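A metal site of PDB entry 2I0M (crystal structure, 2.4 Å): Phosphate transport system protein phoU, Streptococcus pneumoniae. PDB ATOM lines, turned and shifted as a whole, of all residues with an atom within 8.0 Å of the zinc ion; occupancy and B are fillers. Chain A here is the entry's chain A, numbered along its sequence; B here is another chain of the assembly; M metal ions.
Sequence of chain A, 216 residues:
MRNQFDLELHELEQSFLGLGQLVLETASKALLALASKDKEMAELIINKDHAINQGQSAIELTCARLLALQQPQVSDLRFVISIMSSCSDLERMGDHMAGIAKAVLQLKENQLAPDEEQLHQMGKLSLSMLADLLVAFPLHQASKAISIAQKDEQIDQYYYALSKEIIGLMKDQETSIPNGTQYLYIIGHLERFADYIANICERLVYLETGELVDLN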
ATOM      1  N   ASP A  49      25.762  28.829  24.539  1.00  0.00           N
ATOM      2  CA  ASP A  49      25.860  27.613  23.735  1.00  0.00           C
ATOM      3  C   ASP A  49      24.955  27.640  22.482  1.00  0.00           C
ATOM      4  O   ASP A  49      25.366  27.183  21.435  1.00  0.00           O
ATOM      5  CB  ASP A  49      25.622  26.346  24.547  1.00  0.00           C
ATOM      6  CG  ASP A  49      25.923  25.086  23.741  1.00  0.00           C
ATOM      7  OD1 ASP A  49      27.114  24.738  23.560  1.00  0.00           O
ATOM      8  OD2 ASP A  49      24.964  24.459  23.230  1.00  0.00           O
ATOM      9  N   ILE A  52      26.239  28.718  19.083  1.00  0.00           N
ATOM     10  CA  ILE A  52      27.016  27.718  18.338  1.00  0.00           C
ATOM     11  C   ILE A  52      26.059  26.799  17.554  1.00  0.00           C
ATOM     12  O   ILE A  52      26.327  26.438  16.394  1.00  0.00           O
ATOM     13  CB  ILE A  52      27.960  26.892  19.266  1.00  0.00           C
ATOM     14  CG1 ILE A  52      29.000  27.822  19.933  1.00  0.00           C
ATOM     15  CG2 ILE A  52      28.680  25.778  18.453  1.00  0.00           C
ATOM     16  CD1 ILE A  52      29.722  27.246  21.121  1.00  0.00           C
ATOM     17  N   ASN A  53      24.943  26.436  18.180  1.00  0.00           N
ATOM     18  CA  ASN A  53      23.897  25.690  17.496  1.00  0.00           C
ATOM     19  C   ASN A  53      23.454  26.510  16.277  1.00  0.00           C
ATOM     20  O   ASN A  53      23.484  26.001  15.148  1.00  0.00           O
ATOM     21  CB  ASN A  53      22.716  25.435  18.439  1.00  0.00           C
ATOM     22  CG  ASN A  53      22.963  24.318  19.447  1.00  0.00           C
ATOM     23  OD1 ASN A  53      22.055  23.536  19.720  1.00  0.00           O
ATOM     24  ND2 ASN A  53      24.159  24.247  20.018  1.00  0.00           N
ATOM     25  N   GLN A  56      25.975  26.715  13.408  1.00  0.00           N
ATOM     26  CA  GLN A  56      25.976  25.435  12.718  1.00  0.00           C
ATOM     27  C   GLN A  56      24.827  25.335  11.721  1.00  0.00           C
ATOM     28  O   GLN A  56      25.017  24.865  10.605  1.00  0.00           O
ATOM     29  CB  GLN A  56      25.901  24.312  13.751  1.00  0.00           C
ATOM     30  CG  GLN A  56      25.698  22.941  13.147  1.00  0.00           C
ATOM     31  CD  GLN A  56      25.035  21.966  14.094  1.00  0.00           C
ATOM     32  OE1 GLN A  56      24.259  22.354  14.977  1.00  0.00           O
ATOM     33  NE2 GLN A  56      25.308  20.704  13.911  1.00  0.00           N
ATOM     34  N   SER A  88      28.903  20.159  12.622  1.00  0.00           N
ATOM     35  CA  SER A  88      28.234  19.299  13.605  1.00  0.00           C
ATOM     36  C   SER A  88      29.121  18.764  14.747  1.00  0.00           C
ATOM     37  O   SER A  88      28.710  18.764  15.911  1.00  0.00           O
ATOM     38  CB  SER A  88      27.580  18.126  12.882  1.00  0.00           C
ATOM     39  OG  SER A  88      27.074  17.195  13.810  1.00  0.00           O
ATOM     40  N   LEU A  90      31.735  20.195  15.703  1.00  0.00           N
ATOM     41  CA  LEU A  90      32.097  21.411  16.359  1.00  0.00           C
ATOM     42  C   LEU A  90      31.003  21.807  17.363  1.00  0.00           C
ATOM     43  O   LEU A  90      31.318  22.148  18.502  1.00  0.00           O
ATOM     44  CB  LEU A  90      32.339  22.496  15.305  1.00  0.00           C
ATOM     45  CG  LEU A  90      33.580  23.373  15.183  1.00  0.00           C
ATOM     46  CD1 LEU A  90      34.951  22.660  15.338  1.00  0.00           C
ATOM     47  CD2 LEU A  90      33.489  24.097  13.840  1.00  0.00           C
ATOM     48  N   GLU A  91      29.726  21.744  16.985  1.00  0.00           N
ATOM     49  CA  GLU A  91      28.693  22.014  18.008  1.00  0.00           C
ATOM     50  C   GLU A  91      28.619  20.982  19.134  1.00  0.00           C
ATOM     51  O   GLU A  91      28.198  21.315  20.238  1.00  0.00           O
ATOM     52  CB  GLU A  91      27.336  22.576  17.460  1.00  0.00           C
ATOM     53  CG  GLU A  91      26.051  21.788  17.417  1.00  0.00           C
ATOM     54  CD  GLU A  91      25.661  21.002  18.665  1.00  0.00           C
ATOM     55  OE1 GLU A  91      26.129  19.842  18.755  1.00  0.00           O
ATOM     56  OE2 GLU A  91      24.845  21.478  19.494  1.00  0.00           O
ATOM     57  N   ARG A  92      29.093  19.763  18.870  1.00  0.00           N
ATOM     58  CA  ARG A  92      29.169  18.760  19.940  1.00  0.00           C
ATOM     59  C   ARG A  92      30.358  19.054  20.849  1.00  0.00           C
ATOM     60  O   ARG A  92      30.264  18.943  22.067  1.00  0.00           O
ATOM     61  CB  ARG A  92      29.163  17.334  19.377  1.00  0.00           C
ATOM     62  CG  ARG A  92      27.810  17.001  18.730  1.00  0.00           C
ATOM     63  CD  ARG A  92      27.824  15.687  18.033  1.00  0.00           C
ATOM     64  NE  ARG A  92      26.589  15.437  17.283  1.00  0.00           N
ATOM     65  CZ  ARG A  92      26.398  14.380  16.501  1.00  0.00           C
ATOM     66  NH1 ARG A  92      27.371  13.472  16.365  1.00  0.00           N
ATOM     67  NH2 ARG A  92      25.230  14.220  15.863  1.00  0.00           N
ATOM     68  N   MET A  93      31.476  19.477  20.245  1.00  0.00           N
ATOM     69  CA  MET A  93      32.606  20.036  21.007  1.00  0.00           C
ATOM     70  C   MET A  93      32.142  21.154  21.954  1.00  0.00           C
ATOM     71  O   MET A  93      32.350  21.075  23.174  1.00  0.00           O
ATOM     72  CB  MET A  93      33.702  20.510  20.056  1.00  0.00           C
ATOM     73  CG  MET A  93      34.373  19.308  19.350  1.00  0.00           C
ATOM     74  SD  MET A  93      35.440  19.696  17.957  1.00  0.00           S
ATOM     75  CE  MET A  93      36.605  20.698  18.843  1.00  0.00           C
ATOM     76  N   GLY A  94      31.489  22.174  21.389  1.00  0.00           N
ATOM     77  CA  GLY A  94      30.767  23.207  22.139  1.00  0.00           C
ATOM     78  C   GLY A  94      29.901  22.736  23.312  1.00  0.00           C
ATOM     79  O   GLY A  94      30.015  23.264  24.405  1.00  0.00           O
ATOM     80  N   ASP A  95      29.033  21.755  23.095  1.00  0.00           N
ATOM     81  CA  ASP A  95      28.191  21.210  24.173  1.00  0.00           C
ATOM     82  C   ASP A  95      29.019  20.654  25.353  1.00  0.00           C
ATOM     83  O   ASP A  95      28.615  20.752  26.506  1.00  0.00           O
ATOM     84  CB  ASP A  95      27.314  20.075  23.662  1.00  0.00           C
ATOM     85  CG  ASP A  95      26.269  20.519  22.634  1.00  0.00           C
ATOM     86  OD1 ASP A  95      25.811  21.705  22.595  1.00  0.00           O
ATOM     87  OD2 ASP A  95      25.858  19.617  21.880  1.00  0.00           O
ATOM     88  N   HIS A  96      30.157  20.053  25.048  1.00  0.00           N
ATOM     89  CA  HIS A  96      31.021  19.435  26.053  1.00  0.00           C
ATOM     90  C   HIS A  96      31.796  20.470  26.836  1.00  0.00           C
ATOM     91  O   HIS A  96      32.178  20.239  27.978  1.00  0.00           O
ATOM     92  CB  HIS A  96      31.983  18.408  25.409  1.00  0.00           C
ATOM     93  CG  HIS A  96      31.367  17.065  25.208  1.00  0.00           C
ATOM     94  ND1 HIS A  96      31.049  16.572  23.954  1.00  0.00           N
ATOM     95  CD2 HIS A  96      30.953  16.130  26.090  1.00  0.00           C
ATOM     96  CE1 HIS A  96      30.481  15.387  24.081  1.00  0.00           C
ATOM     97  NE2 HIS A  96      30.414  15.096  25.367  1.00  0.00           N
ATOM     98  N   ASN B 199      22.287  11.490  19.976  1.00  0.00           N
ATOM     99  CA  ASN B 199      22.524  12.417  18.896  1.00  0.00           C
ATOM    100  C   ASN B 199      21.570  12.247  17.698  1.00  0.00           C
ATOM    101  O   ASN B 199      21.115  13.239  17.151  1.00  0.00           O
ATOM    102  CB  ASN B 199      23.981  12.358  18.444  1.00  0.00           C
ATOM    103  CG  ASN B 199      24.958  13.026  19.430  1.00  0.00           C
ATOM    104  OD1 ASN B 199      26.137  12.646  19.524  1.00  0.00           O
ATOM    105  ND2 ASN B 199      24.463  14.024  20.161  1.00  0.00           N
ATOM    106  N   GLU B 202      18.148  13.631  18.783  1.00  0.00           N
ATOM    107  CA  GLU B 202      18.095  15.099  18.737  1.00  0.00           C
ATOM    108  C   GLU B 202      17.892  15.638  17.318  1.00  0.00           C
ATOM    109  O   GLU B 202      17.148  16.593  17.114  1.00  0.00           O
ATOM    110  CB  GLU B 202      19.360  15.723  19.314  1.00  0.00           C
ATOM    111  CG  GLU B 202      19.636  15.365  20.775  1.00  0.00           C
ATOM    112  CD  GLU B 202      20.847  16.095  21.346  1.00  0.00           C
ATOM    113  OE1 GLU B 202      20.708  16.774  22.377  1.00  0.00           O
ATOM    114  OE2 GLU B 202      21.953  15.990  20.769  1.00  0.00           O
ATOM    115  N   LEU B 212      17.768  22.488  16.344  1.00  0.00           N
ATOM    116  CA  LEU B 212      18.532  21.480  17.065  1.00  0.00           C
ATOM    117  C   LEU B 212      18.635  21.943  18.513  1.00  0.00           C
ATOM    118  O   LEU B 212      19.135  23.039  18.786  1.00  0.00           O
ATOM    119  CB  LEU B 212      19.915  21.268  16.434  1.00  0.00           C
ATOM    120  CG  LEU B 212      20.712  20.002  16.804  1.00  0.00           C
ATOM    121  CD1 LEU B 212      19.979  18.690  16.431  1.00  0.00           C
ATOM    122  CD2 LEU B 212      22.131  20.025  16.205  1.00  0.00           C
ATOM    123  N   VAL B 213      18.090  21.145  19.428  1.00  0.00           N
ATOM    124  CA  VAL B 213      18.142  21.448  20.843  1.00  0.00           C
ATOM    125  C   VAL B 213      19.016  20.409  21.534  1.00  0.00           C
ATOM    126  O   VAL B 213      19.177  19.293  21.018  1.00  0.00           O
ATOM    127  CB  VAL B 213      16.722  21.495  21.515  1.00  0.00           C
ATOM    128  CG1 VAL B 213      15.692  22.181  20.609  1.00  0.00           C
ATOM    129  CG2 VAL B 213      16.242  20.099  21.924  1.00  0.00           C
ATOM    130  N   ASP B 214      19.578  20.761  22.676  1.00  0.00           N
ATOM    131  CA  ASP B 214      20.467  19.836  23.371  1.00  0.00           C
ATOM    132  C   ASP B 214      19.750  19.063  24.485  1.00  0.00           C
ATOM    133  O   ASP B 214      19.065  19.664  25.337  1.00  0.00           O
ATOM    134  CB  ASP B 214      21.716  20.583  23.855  1.00  0.00           C
ATOM    135  CG  ASP B 214      22.496  21.183  22.707  1.00  0.00           C
ATOM    136  OD1 ASP B 214      23.074  20.418  21.911  1.00  0.00           O
ATOM    137  OD2 ASP B 214      22.526  22.417  22.573  1.00  0.00           O
ATOM    138  N   LEU B 215      19.899  17.744  24.451  1.00  0.00           N
ATOM    139  CA  LEU B 215      19.217  16.848  25.391  1.00  0.00           C
ATOM    140  C   LEU B 215      20.230  16.112  26.283  1.00  0.00           C
ATOM    141  O   LEU B 215      21.037  15.303  25.805  1.00  0.00           O
ATOM    142  CB  LEU B 215      18.312  15.834  24.641  1.00  0.00           C
ATOM    143  CG  LEU B 215      17.235  16.287  23.640  1.00  0.00           C
ATOM    144  CD1 LEU B 215      16.654  15.099  22.873  1.00  0.00           C
ATOM    145  CD2 LEU B 215      16.100  17.067  24.286  1.00  0.00           C
HETATM  146 ZN    ZN M   1      24.320  19.544  20.574  1.00  0.00          ZN
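The side-chain amide oxygen (OD1) of Asn 53 sits close to the side-chain carboxylate (OD2) of Asp 214 of chain B (3.1 Å). The side-chain carboxylate (OE2) of Glu 91 sits close to the side-chain amide nitrogen (ND2) of Asn 53 (2.9 Å).
Three residues have an atom within 4 Å of the zinc ion: Glu 91, Asp 95 and Asp 214 of chain B. Along chain A the residues within 4 Å of the zinc ion span positions 91 to 95. The nearest printed residue that does not touch the zinc ion is Glu 202 of chain B (4.3 Å).
The zinc ion is bound by OD2 of Asp 95 (2.0 Å), OD1 of Asp 214 of chain B (2.0 Å), OE2 of Glu 91 (2.3 Å) and OE1 of Glu 91 (2.6 Å). The zinc ion has four donor atoms within binding distance.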
